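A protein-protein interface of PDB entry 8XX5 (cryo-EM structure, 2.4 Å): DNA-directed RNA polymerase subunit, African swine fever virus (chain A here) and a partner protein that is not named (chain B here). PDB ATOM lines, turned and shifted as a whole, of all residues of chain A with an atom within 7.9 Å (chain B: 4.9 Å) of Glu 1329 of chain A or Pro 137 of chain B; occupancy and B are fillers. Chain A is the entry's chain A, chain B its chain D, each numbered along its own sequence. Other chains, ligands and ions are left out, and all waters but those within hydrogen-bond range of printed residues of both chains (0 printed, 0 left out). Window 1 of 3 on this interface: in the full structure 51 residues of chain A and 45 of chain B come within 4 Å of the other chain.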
ATOM      1  N   GLU A 857     -24.755  23.825  21.807  1.00  0.00           N
ATOM      2  CA  GLU A 857     -24.489  23.707  23.236  1.00  0.00           C
ATOM      3  C   GLU A 857     -24.773  24.998  23.991  1.00  0.00           C
ATOM      4  O   GLU A 857     -24.594  25.036  25.213  1.00  0.00           O
ATOM      5  CB  GLU A 857     -23.052  23.250  23.524  1.00  0.00           C
ATOM      6  CG  GLU A 857     -22.906  21.744  23.597  1.00  0.00           C
ATOM      7  CD  GLU A 857     -21.689  21.234  22.857  1.00  0.00           C
ATOM      8  OE1 GLU A 857     -20.676  21.960  22.801  1.00  0.00           O
ATOM      9  OE2 GLU A 857     -21.745  20.103  22.334  1.00  0.00           O
ATOM     10  N   ASN A 914      -7.700  21.285  29.130  1.00  0.00           N
ATOM     11  CA  ASN A 914      -8.067  19.947  28.689  1.00  0.00           C
ATOM     12  C   ASN A 914      -8.314  19.922  27.188  1.00  0.00           C
ATOM     13  O   ASN A 914      -7.922  18.971  26.502  1.00  0.00           O
ATOM     14  CB  ASN A 914      -9.300  19.462  29.449  1.00  0.00           C
ATOM     15  CG  ASN A 914      -9.598  18.000  29.201  1.00  0.00           C
ATOM     16  OD1 ASN A 914     -10.302  17.652  28.255  1.00  0.00           O
ATOM     17  ND2 ASN A 914      -9.062  17.135  30.050  1.00  0.00           N
ATOM     18  N   PHE A 918      -6.257  17.307  23.897  1.00  0.00           N
ATOM     19  CA  PHE A 918      -6.703  16.389  22.855  1.00  0.00           C
ATOM     20  C   PHE A 918      -6.781  17.068  21.491  1.00  0.00           C
ATOM     21  O   PHE A 918      -7.597  16.694  20.646  1.00  0.00           O
ATOM     22  CB  PHE A 918      -8.038  15.732  23.218  1.00  0.00           C
ATOM     23  CG  PHE A 918      -9.153  16.696  23.537  1.00  0.00           C
ATOM     24  CD1 PHE A 918      -9.850  17.339  22.529  1.00  0.00           C
ATOM     25  CD2 PHE A 918      -9.539  16.912  24.848  1.00  0.00           C
ATOM     26  CE1 PHE A 918     -10.882  18.205  22.823  1.00  0.00           C
ATOM     27  CE2 PHE A 918     -10.573  17.775  25.145  1.00  0.00           C
ATOM     28  CZ  PHE A 918     -11.245  18.421  24.132  1.00  0.00           C
ATOM     29  N   THR A1322      -9.645   6.795  17.441  1.00  0.00           N
ATOM     30  CA  THR A1322     -10.128   7.433  18.661  1.00  0.00           C
ATOM     31  C   THR A1322     -11.415   6.786  19.151  1.00  0.00           C
ATOM     32  O   THR A1322     -11.577   6.536  20.350  1.00  0.00           O
ATOM     33  CB  THR A1322     -10.347   8.926  18.412  1.00  0.00           C
ATOM     34  OG1 THR A1322      -9.237   9.458  17.681  1.00  0.00           O
ATOM     35  CG2 THR A1322     -10.497   9.673  19.723  1.00  0.00           C
ATOM     36  N   MET A1323     -12.346   6.510  18.235  1.00  0.00           N
ATOM     37  CA  MET A1323     -13.598   5.869  18.619  1.00  0.00           C
ATOM     38  C   MET A1323     -13.342   4.485  19.202  1.00  0.00           C
ATOM     39  O   MET A1323     -13.889   4.127  20.252  1.00  0.00           O
ATOM     40  CB  MET A1323     -14.523   5.783  17.404  1.00  0.00           C
ATOM     41  CG  MET A1323     -15.702   4.836  17.555  1.00  0.00           C
ATOM     42  SD  MET A1323     -16.595   5.007  19.108  1.00  0.00           S
ATOM     43  CE  MET A1323     -18.188   4.357  18.637  1.00  0.00           C
ATOM     44  N   TYR A1326     -11.124   5.236  22.599  1.00  0.00           N
ATOM     45  CA  TYR A1326     -11.559   6.189  23.614  1.00  0.00           C
ATOM     46  C   TYR A1326     -13.067   6.221  23.819  1.00  0.00           C
ATOM     47  O   TYR A1326     -13.524   6.285  24.963  1.00  0.00           O
ATOM     48  CB  TYR A1326     -11.055   7.591  23.266  1.00  0.00           C
ATOM     49  CG  TYR A1326      -9.563   7.751  23.413  1.00  0.00           C
ATOM     50  CD1 TYR A1326      -8.849   6.984  24.322  1.00  0.00           C
ATOM     51  CD2 TYR A1326      -8.865   8.670  22.644  1.00  0.00           C
ATOM     52  CE1 TYR A1326      -7.484   7.126  24.458  1.00  0.00           C
ATOM     53  CE2 TYR A1326      -7.501   8.819  22.773  1.00  0.00           C
ATOM     54  CZ  TYR A1326      -6.816   8.046  23.682  1.00  0.00           C
ATOM     55  OH  TYR A1326      -5.454   8.195  23.813  1.00  0.00           O
ATOM     56  N   GLY A1327     -13.858   6.181  22.753  1.00  0.00           N
ATOM     57  CA  GLY A1327     -15.299   6.139  22.867  1.00  0.00           C
ATOM     58  C   GLY A1327     -15.973   7.091  21.904  1.00  0.00           C
ATOM     59  O   GLY A1327     -15.335   7.780  21.111  1.00  0.00           O
ATOM     60  N   ILE A1328     -17.304   7.121  21.991  1.00  0.00           N
ATOM     61  CA  ILE A1328     -18.096   7.918  21.058  1.00  0.00           C
ATOM     62  C   ILE A1328     -17.968   9.409  21.351  1.00  0.00           C
ATOM     63  O   ILE A1328     -18.013  10.228  20.429  1.00  0.00           O
ATOM     64  CB  ILE A1328     -19.567   7.454  21.069  1.00  0.00           C
ATOM     65  CG1 ILE A1328     -20.321   8.046  19.877  1.00  0.00           C
ATOM     66  CG2 ILE A1328     -20.254   7.809  22.379  1.00  0.00           C
ATOM     67  CD1 ILE A1328     -19.727   7.681  18.539  1.00  0.00           C
ATOM     68  N   GLU A1329     -17.818   9.793  22.619  1.00  0.00           N
ATOM     69  CA  GLU A1329     -17.683  11.211  22.947  1.00  0.00           C
ATOM     70  C   GLU A1329     -16.348  11.762  22.463  1.00  0.00           C
ATOM     71  O   GLU A1329     -16.284  12.848  21.871  1.00  0.00           O
ATOM     72  CB  GLU A1329     -17.839  11.411  24.452  1.00  0.00           C
ATOM     73  CG  GLU A1329     -19.263  11.284  24.947  1.00  0.00           C
ATOM     74  CD  GLU A1329     -20.153  12.411  24.462  1.00  0.00           C
ATOM     75  OE1 GLU A1329     -19.746  13.585  24.585  1.00  0.00           O
ATOM     76  OE2 GLU A1329     -21.259  12.126  23.961  1.00  0.00           O
ATOM     77  N   ALA A1330     -15.266  11.021  22.709  1.00  0.00           N
ATOM     78  CA  ALA A1330     -13.972  11.418  22.172  1.00  0.00           C
ATOM     79  C   ALA A1330     -13.970  11.372  20.654  1.00  0.00           C
ATOM     80  O   ALA A1330     -13.305  12.188  20.012  1.00  0.00           O
ATOM     81  CB  ALA A1330     -12.870  10.526  22.738  1.00  0.00           C
ATOM     82  N   ALA A1331     -14.713  10.436  20.060  1.00  0.00           N
ATOM     83  CA  ALA A1331     -14.848  10.412  18.608  1.00  0.00           C
ATOM     84  C   ALA A1331     -15.559  11.660  18.101  1.00  0.00           C
ATOM     85  O   ALA A1331     -15.207  12.199  17.048  1.00  0.00           O
ATOM     86  CB  ALA A1331     -15.594   9.155  18.167  1.00  0.00           C
ATOM     87  N   ARG A1332     -16.575  12.123  18.831  1.00  0.00           N
ATOM     88  CA  ARG A1332     -17.264  13.356  18.465  1.00  0.00           C
ATOM     89  C   ARG A1332     -16.322  14.552  18.540  1.00  0.00           C
ATOM     90  O   ARG A1332     -16.293  15.400  17.637  1.00  0.00           O
ATOM     91  CB  ARG A1332     -18.470  13.555  19.383  1.00  0.00           C
ATOM     92  CG  ARG A1332     -19.284  14.797  19.104  1.00  0.00           C
ATOM     93  CD  ARG A1332     -20.285  15.041  20.214  1.00  0.00           C
ATOM     94  NE  ARG A1332     -20.619  16.452  20.348  1.00  0.00           N
ATOM     95  CZ  ARG A1332     -19.949  17.312  21.102  1.00  0.00           C
ATOM     96  NH1 ARG A1332     -18.891  16.939  21.802  1.00  0.00           N
ATOM     97  NH2 ARG A1332     -20.351  18.577  21.156  1.00  0.00           N
ATOM     98  N   GLN A1333     -15.534  14.629  19.614  1.00  0.00           N
ATOM     99  CA  GLN A1333     -14.558  15.709  19.730  1.00  0.00           C
ATOM    100  C   GLN A1333     -13.518  15.632  18.620  1.00  0.00           C
ATOM    101  O   GLN A1333     -13.071  16.662  18.101  1.00  0.00           O
ATOM    102  CB  GLN A1333     -13.888  15.672  21.102  1.00  0.00           C
ATOM    103  CG  GLN A1333     -14.819  15.992  22.255  1.00  0.00           C
ATOM    104  CD  GLN A1333     -15.054  17.482  22.426  1.00  0.00           C
ATOM    105  OE1 GLN A1333     -14.705  18.284  21.560  1.00  0.00           O
ATOM    106  NE2 GLN A1333     -15.652  17.858  23.549  1.00  0.00           N
ATOM    107  N   LYS A1334     -13.126  14.417  18.238  1.00  0.00           N
ATOM    108  CA  LYS A1334     -12.165  14.246  17.156  1.00  0.00           C
ATOM    109  C   LYS A1334     -12.755  14.665  15.816  1.00  0.00           C
ATOM    110  O   LYS A1334     -12.056  15.245  14.982  1.00  0.00           O
ATOM    111  CB  LYS A1334     -11.690  12.795  17.101  1.00  0.00           C
ATOM    112  CG  LYS A1334     -10.563  12.558  16.116  1.00  0.00           C
ATOM    113  CD  LYS A1334      -9.343  13.378  16.483  1.00  0.00           C
ATOM    114  CE  LYS A1334      -8.894  13.097  17.909  1.00  0.00           C
ATOM    115  NZ  LYS A1334      -7.649  13.831  18.248  1.00  0.00           N
ATOM    116  N   ILE A1335     -14.032  14.360  15.585  1.00  0.00           N
ATOM    117  CA  ILE A1335     -14.698  14.828  14.373  1.00  0.00           C
ATOM    118  C   ILE A1335     -14.702  16.348  14.336  1.00  0.00           C
ATOM    119  O   ILE A1335     -14.405  16.962  13.303  1.00  0.00           O
ATOM    120  CB  ILE A1335     -16.126  14.257  14.286  1.00  0.00           C
ATOM    121  CG1 ILE A1335     -16.090  12.749  14.053  1.00  0.00           C
ATOM    122  CG2 ILE A1335     -16.908  14.937  13.177  1.00  0.00           C
ATOM    123  CD1 ILE A1335     -17.404  12.062  14.336  1.00  0.00           C
ATOM    124  N   ILE A1336     -15.022  16.977  15.470  1.00  0.00           N
ATOM    125  CA  ILE A1336     -14.993  18.436  15.550  1.00  0.00           C
ATOM    126  C   ILE A1336     -13.609  18.959  15.187  1.00  0.00           C
ATOM    127  O   ILE A1336     -13.463  19.854  14.345  1.00  0.00           O
ATOM    128  CB  ILE A1336     -15.414  18.907  16.952  1.00  0.00           C
ATOM    129  CG1 ILE A1336     -16.903  18.666  17.186  1.00  0.00           C
ATOM    130  CG2 ILE A1336     -15.085  20.373  17.135  1.00  0.00           C
ATOM    131  CD1 ILE A1336     -17.253  18.413  18.633  1.00  0.00           C
ATOM    132  N   ALA A1357     -20.747  16.864  14.053  1.00  0.00           N
ATOM    133  CA  ALA A1357     -20.246  15.795  14.910  1.00  0.00           C
ATOM    134  C   ALA A1357     -21.371  15.112  15.677  1.00  0.00           C
ATOM    135  O   ALA A1357     -21.334  13.895  15.888  1.00  0.00           O
ATOM    136  CB  ALA A1357     -19.198  16.345  15.871  1.00  0.00           C
ATOM    137  N   ASP A1358     -22.372  15.876  16.114  1.00  0.00           N
ATOM    138  CA  ASP A1358     -23.465  15.309  16.890  1.00  0.00           C
ATOM    139  C   ASP A1358     -24.420  14.505  16.025  1.00  0.00           C
ATOM    140  O   ASP A1358     -25.004  13.527  16.503  1.00  0.00           O
ATOM    141  CB  ASP A1358     -24.221  16.420  17.617  1.00  0.00           C
ATOM    142  CG  ASP A1358     -23.663  16.695  18.998  1.00  0.00           C
ATOM    143  OD1 ASP A1358     -23.913  15.883  19.912  1.00  0.00           O
ATOM    144  OD2 ASP A1358     -22.976  17.722  19.169  1.00  0.00           O
ATOM    145  N   THR A1361     -22.628  11.058  15.504  1.00  0.00           N
ATOM    146  CA  THR A1361     -22.374  10.239  16.685  1.00  0.00           C
ATOM    147  C   THR A1361     -23.621  10.047  17.542  1.00  0.00           C
ATOM    148  O   THR A1361     -23.513   9.626  18.697  1.00  0.00           O
ATOM    149  CB  THR A1361     -21.252  10.850  17.529  1.00  0.00           C
ATOM    150  OG1 THR A1361     -21.595  12.195  17.881  1.00  0.00           O
ATOM    151  CG2 THR A1361     -19.942  10.853  16.757  1.00  0.00           C
ATOM    152  N   GLY A1364     -24.400   6.361  18.965  1.00  0.00           N
ATOM    153  CA  GLY A1364     -23.350   5.675  19.679  1.00  0.00           C
ATOM    154  C   GLY A1364     -22.250   5.130  18.801  1.00  0.00           C
ATOM    155  O   GLY A1364     -21.260   4.611  19.326  1.00  0.00           O
ATOM    156  N   VAL A1366     -19.942   6.006  14.979  1.00  0.00           N
ATOM    157  CA  VAL A1366     -19.581   7.056  14.032  1.00  0.00           C
ATOM    158  C   VAL A1366     -20.214   6.695  12.692  1.00  0.00           C
ATOM    159  O   VAL A1366     -19.659   5.914  11.918  1.00  0.00           O
ATOM    160  CB  VAL A1366     -18.066   7.229  13.915  1.00  0.00           C
ATOM    161  CG1 VAL A1366     -17.741   8.354  12.951  1.00  0.00           C
ATOM    162  CG2 VAL A1366     -17.461   7.502  15.281  1.00  0.00           C
ATOM    163  N   ALA B 135      -8.862  13.168  26.370  1.00  0.00           N
ATOM    164  CA  ALA B 135      -9.847  13.254  25.298  1.00  0.00           C
ATOM    165  C   ALA B 135     -11.220  12.749  25.719  1.00  0.00           C
ATOM    166  O   ALA B 135     -12.212  13.076  25.060  1.00  0.00           O
ATOM    167  CB  ALA B 135      -9.365  12.471  24.076  1.00  0.00           C
ATOM    168  N   ILE B 136     -11.303  11.971  26.791  1.00  0.00           N
ATOM    169  CA  ILE B 136     -12.555  11.364  27.226  1.00  0.00           C
ATOM    170  C   ILE B 136     -13.201  12.290  28.255  1.00  0.00           C
ATOM    171  O   ILE B 136     -12.592  12.544  29.305  1.00  0.00           O
ATOM    172  CB  ILE B 136     -12.323   9.968  27.816  1.00  0.00           C
ATOM    173  CG1 ILE B 136     -11.958   8.981  26.707  1.00  0.00           C
ATOM    174  CG2 ILE B 136     -13.551   9.498  28.573  1.00  0.00           C
ATOM    175  CD1 ILE B 136     -11.421   7.668  27.216  1.00  0.00           C
ATOM    176  N   PRO B 137     -14.399  12.808  28.002  1.00  0.00           N
ATOM    177  CA  PRO B 137     -15.071  13.641  29.002  1.00  0.00           C
ATOM    178  C   PRO B 137     -15.595  12.798  30.153  1.00  0.00           C
ATOM    179  O   PRO B 137     -15.637  11.569  30.102  1.00  0.00           O
ATOM    180  CB  PRO B 137     -16.212  14.292  28.218  1.00  0.00           C
ATOM    181  CG  PRO B 137     -16.487  13.344  27.114  1.00  0.00           C
ATOM    182  CD  PRO B 137     -15.178  12.700  26.756  1.00  0.00           C
ATOM    183  N   LYS B 138     -15.999  13.489  31.215  1.00  0.00           N
ATOM    184  CA  LYS B 138     -16.459  12.812  32.419  1.00  0.00           C
ATOM    185  C   LYS B 138     -17.819  12.170  32.176  1.00  0.00           C
ATOM    186  O   LYS B 138     -18.802  12.864  31.896  1.00  0.00           O
ATOM    187  CB  LYS B 138     -16.529  13.797  33.582  1.00  0.00           C
ATOM    188  CG  LYS B 138     -15.520  13.527  34.684  1.00  0.00           C
ATOM    189  CD  LYS B 138     -14.178  13.087  34.118  1.00  0.00           C
ATOM    190  CE  LYS B 138     -13.073  13.213  35.152  1.00  0.00           C
ATOM    191  NZ  LYS B 138     -11.850  12.465  34.748  1.00  0.00           N
ATOM    192  N   HIS B 139     -17.871  10.846  32.278  1.00  0.00           N
ATOM    193  CA  HIS B 139     -19.115  10.095  32.211  1.00  0.00           C
ATOM    194  C   HIS B 139     -19.546   9.718  33.620  1.00  0.00           C
ATOM    195  O   HIS B 139     -18.713   9.367  34.460  1.00  0.00           O
ATOM    196  CB  HIS B 139     -18.961   8.827  31.367  1.00  0.00           C
ATOM    197  CG  HIS B 139     -18.596   9.079  29.939  1.00  0.00           C
ATOM    198  ND1 HIS B 139     -17.512   9.843  29.566  1.00  0.00           N
ATOM    199  CD2 HIS B 139     -19.168   8.652  28.788  1.00  0.00           C
ATOM    200  CE1 HIS B 139     -17.435   9.882  28.248  1.00  0.00           C
ATOM    201  NE2 HIS B 139     -18.428   9.169  27.752  1.00  0.00           N
ATOM    202  N   ILE B 184     -22.994  12.985  30.772  1.00  0.00           N
ATOM    203  CA  ILE B 184     -21.658  13.276  30.267  1.00  0.00           C
ATOM    204  C   ILE B 184     -21.438  14.780  30.318  1.00  0.00           C
ATOM    205  O   ILE B 184     -22.208  15.547  29.727  1.00  0.00           O
ATOM    206  CB  ILE B 184     -21.463  12.739  28.842  1.00  0.00           C
ATOM    207  CG1 ILE B 184     -22.058  11.335  28.730  1.00  0.00           C
ATOM    208  CG2 ILE B 184     -19.992  12.737  28.473  1.00  0.00           C
ATOM    209  CD1 ILE B 184     -21.724  10.624  27.452  1.00  0.00           C
ATOM    210  N   GLU B 185     -20.388  15.199  31.020  1.00  0.00           N
ATOM    211  CA  GLU B 185     -19.986  16.603  31.081  1.00  0.00           C
ATOM    212  C   GLU B 185     -18.950  16.834  29.990  1.00  0.00           C
ATOM    213  O   GLU B 185     -17.755  16.603  30.177  1.00  0.00           O
ATOM    214  CB  GLU B 185     -19.440  16.950  32.460  1.00  0.00           C
ATOM    215  CG  GLU B 185     -20.398  17.733  33.338  1.00  0.00           C
ATOM    216  CD  GLU B 185     -20.318  19.231  33.108  1.00  0.00           C
ATOM    217  OE1 GLU B 185     -19.744  19.651  32.081  1.00  0.00           O
ATOM    218  OE2 GLU B 185     -20.824  19.990  33.960  1.00  0.00           O
ATOM    219  N   ARG B 186     -19.413  17.295  28.834  1.00  0.00           N
ATOM    220  CA  ARG B 186     -18.439  17.422  27.763  1.00  0.00           C
ATOM    221  C   ARG B 186     -17.913  18.847  27.673  1.00  0.00           C
ATOM    222  O   ARG B 186     -18.690  19.802  27.777  1.00  0.00           O
ATOM    223  CB  ARG B 186     -19.053  17.031  26.419  1.00  0.00           C
ATOM    224  CG  ARG B 186     -20.502  17.437  26.265  1.00  0.00           C
ATOM    225  CD  ARG B 186     -20.953  17.347  24.819  1.00  0.00           C
ATOM    226  NE  ARG B 186     -21.305  15.985  24.437  1.00  0.00           N
ATOM    227  CZ  ARG B 186     -22.256  15.676  23.567  1.00  0.00           C
ATOM    228  NH1 ARG B 186     -22.976  16.611  22.968  1.00  0.00           N
ATOM    229  NH2 ARG B 186     -22.492  14.397  23.291  1.00  0.00           N
ATOM    230  N   PRO B 187     -16.604  19.014  27.494  1.00  0.00           N
ATOM    231  CA  PRO B 187     -16.065  20.354  27.239  1.00  0.00           C
ATOM    232  C   PRO B 187     -16.650  20.936  25.964  1.00  0.00           C
ATOM    233  O   PRO B 187     -16.888  20.225  24.985  1.00  0.00           O
ATOM    234  CB  PRO B 187     -14.556  20.114  27.111  1.00  0.00           C
ATOM    235  CG  PRO B 187     -14.314  18.808  27.788  1.00  0.00           C
ATOM    236  CD  PRO B 187     -15.547  17.994  27.568  1.00  0.00           C
ATOM    237  N   VAL B 196     -24.818  16.418  28.767  1.00  0.00           N
ATOM    238  CA  VAL B 196     -25.609  15.611  27.849  1.00  0.00           C
ATOM    239  C   VAL B 196     -25.913  14.284  28.529  1.00  0.00           C
ATOM    240  O   VAL B 196     -25.078  13.745  29.263  1.00  0.00           O
ATOM    241  CB  VAL B 196     -24.876  15.414  26.502  1.00  0.00           C
ATOM    242  CG1 VAL B 196     -24.775  13.941  26.127  1.00  0.00           C
ATOM    243  CG2 VAL B 196     -25.561  16.208  25.407  1.00  0.00           C
ATOM    244  N   ARG B 198     -27.088  10.386  27.758  1.00  0.00           N
ATOM    245  CA  ARG B 198     -27.159   9.387  26.705  1.00  0.00           C
ATOM    246  C   ARG B 198     -27.763   8.098  27.241  1.00  0.00           C
ATOM    247  O   ARG B 198     -27.654   7.786  28.430  1.00  0.00           O
ATOM    248  CB  ARG B 198     -25.777   9.105  26.107  1.00  0.00           C
ATOM    249  CG  ARG B 198     -25.172  10.285  25.374  1.00  0.00           C
ATOM    250  CD  ARG B 198     -23.928   9.884  24.605  1.00  0.00           C
ATOM    251  NE  ARG B 198     -24.244   9.380  23.275  1.00  0.00           N
ATOM    252  CZ  ARG B 198     -23.860   9.959  22.146  1.00  0.00           C
ATOM    253  NH1 ARG B 198     -23.151  11.075  22.147  1.00  0.00           N
ATOM    254  NH2 ARG B 198     -24.200   9.405  20.986  1.00  0.00           N
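NE2 of Gln 1333 of chain A lies within hydrogen-bond range of O of Pro 187 of chain B (3.0 Å).
OD1 of Asp 1358 of chain A lies within salt-bridge range of NH1 of Arg 186 of chain B.
NH2 of Arg 198 of chain B lies within hydrogen-bond range of O of Thr 1361 of chain A (2.4 Å).
The guanidinium group of Arg 198 of chain B lies within salt-bridge range of the side-chain carboxylate of Glu 1329 of chain A.
The guanidinium group (NH1) of Arg 186 of chain B lies within salt-bridge range of the side-chain carboxylate (OE2) of Glu 857 of chain A (3.8 Å).
The side-chain carboxylate (OE2) of Glu 1329 of chain A is in salt-bridge range of the guanidinium group (NH2) of Arg 186 of chain B, 2.7 Å away.
The backbone carbonyl oxygen (O) of Ala 1357 of chain A is in hydrogen-bond range of the side-chain hydroxyl (OG1) of Thr 1361 of chain A (2.6 Å).
O of Val 196 of chain B sits at hydrogen-bond distance from N of Ile 184 of chain B (2.7 Å).
O of Pro 137 of chain B sits at hydrogen-bond distance from ND1 of His 139 of chain B (2.6 Å).
The side-chain carboxylate of Glu 857 of chain A lies within salt-bridge range of the guanidinium group of Arg 1332 of chain A, at 3.8 Å.
The guanidinium group (NE) of Arg 1332 of chain A lies within salt-bridge range of the side-chain carboxylate (OD2) of Asp 1358 of chain A (2.9 Å).
CB of Ala 135 of chain B touches CB of Phe 918 of chain A (3.6 Å).
CD1 of Ile 136 of chain B touches O of Tyr 1326 of chain A, at 3.4 Å.
Glu 1329 of chain A touches Pro 137 of chain B (CB to CG, 3.6 Å).
NE2 of His 139 of chain B touches CG of Glu 1329 of chain A, at 3.6 Å.
Ile 184 of chain B touches Glu 1329 of chain A.
Ala 1330 of chain A touches Ala 135 of chain B.
Arg 186 of chain B touches Arg 1332 of chain A.
Arg 198 of chain B touches Gly 1364 of chain A (NH2 to N, 3.7 Å).
Of chain B, only Pro 137 (3.6 Å), His 139 (3.6 Å), Ile 184 (3.6 Å), Arg 186 (2.7 Å) and Arg 198 (2.8 Å) come within 4 Å of Glu 1329 of chain A.
Printed residues of chain B within 4 Å of Gln 1333 of chain A: Pro 187.
Ile 1335 of chain A touches none of the printed residues of chain B.
Printed residues of chain B within 4 Å of Asp 1358 of chain A: Arg 186 (3.3 Å).
Printed residues of chain B within 4 Å of Thr 1361 of chain A: Arg 198.
Printed residues of chain A within 4 Å of Ala 135 of chain B: Phe 918 (3.6 Å) and Ala 1330 (3.5 Å).
Of the printed residues of chain A, Ile 136 of chain B touches Tyr 1326 (3.4 Å).
Lys 138 of chain B touches none of the printed residues of chain A.
The nearest residue of chain B that does not touch Glu 1329 of chain A is Val 196 of chain B (4.5 Å).
The nearest printed residue of chain B that does not touch Gln 1333 of chain A is Arg 186 of chain B (4.5 Å).
Of the 21 printed residues of chain A, 10 touch a printed residue of chain B.
Hydrophobic or aromatic side chains of chain A within 4 Å of the printed part of chain B: Phe 918, Tyr 1326 and Ala 1330.
Of the 11 printed residues of chain B, 8 touch a printed residue of chain A.
Hydrophobic or aromatic side chains of chain B within 4 Å of the printed part of chain A: Ala 135, Ile 136, Pro 137, His 139 and Ile 184.
Among the printed residues, Asp or Glu carboxylates within 4 Å of a Lys or Arg side-chain nitrogen of the other chain: Glu 857 of chain A with Arg 186 of chain B, Glu 1329 of chain A with Arg 186 of chain B, Glu 1329 of chain A with Arg 198 of chain B and Asp 1358 of chain A with Arg 186 of chain B.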
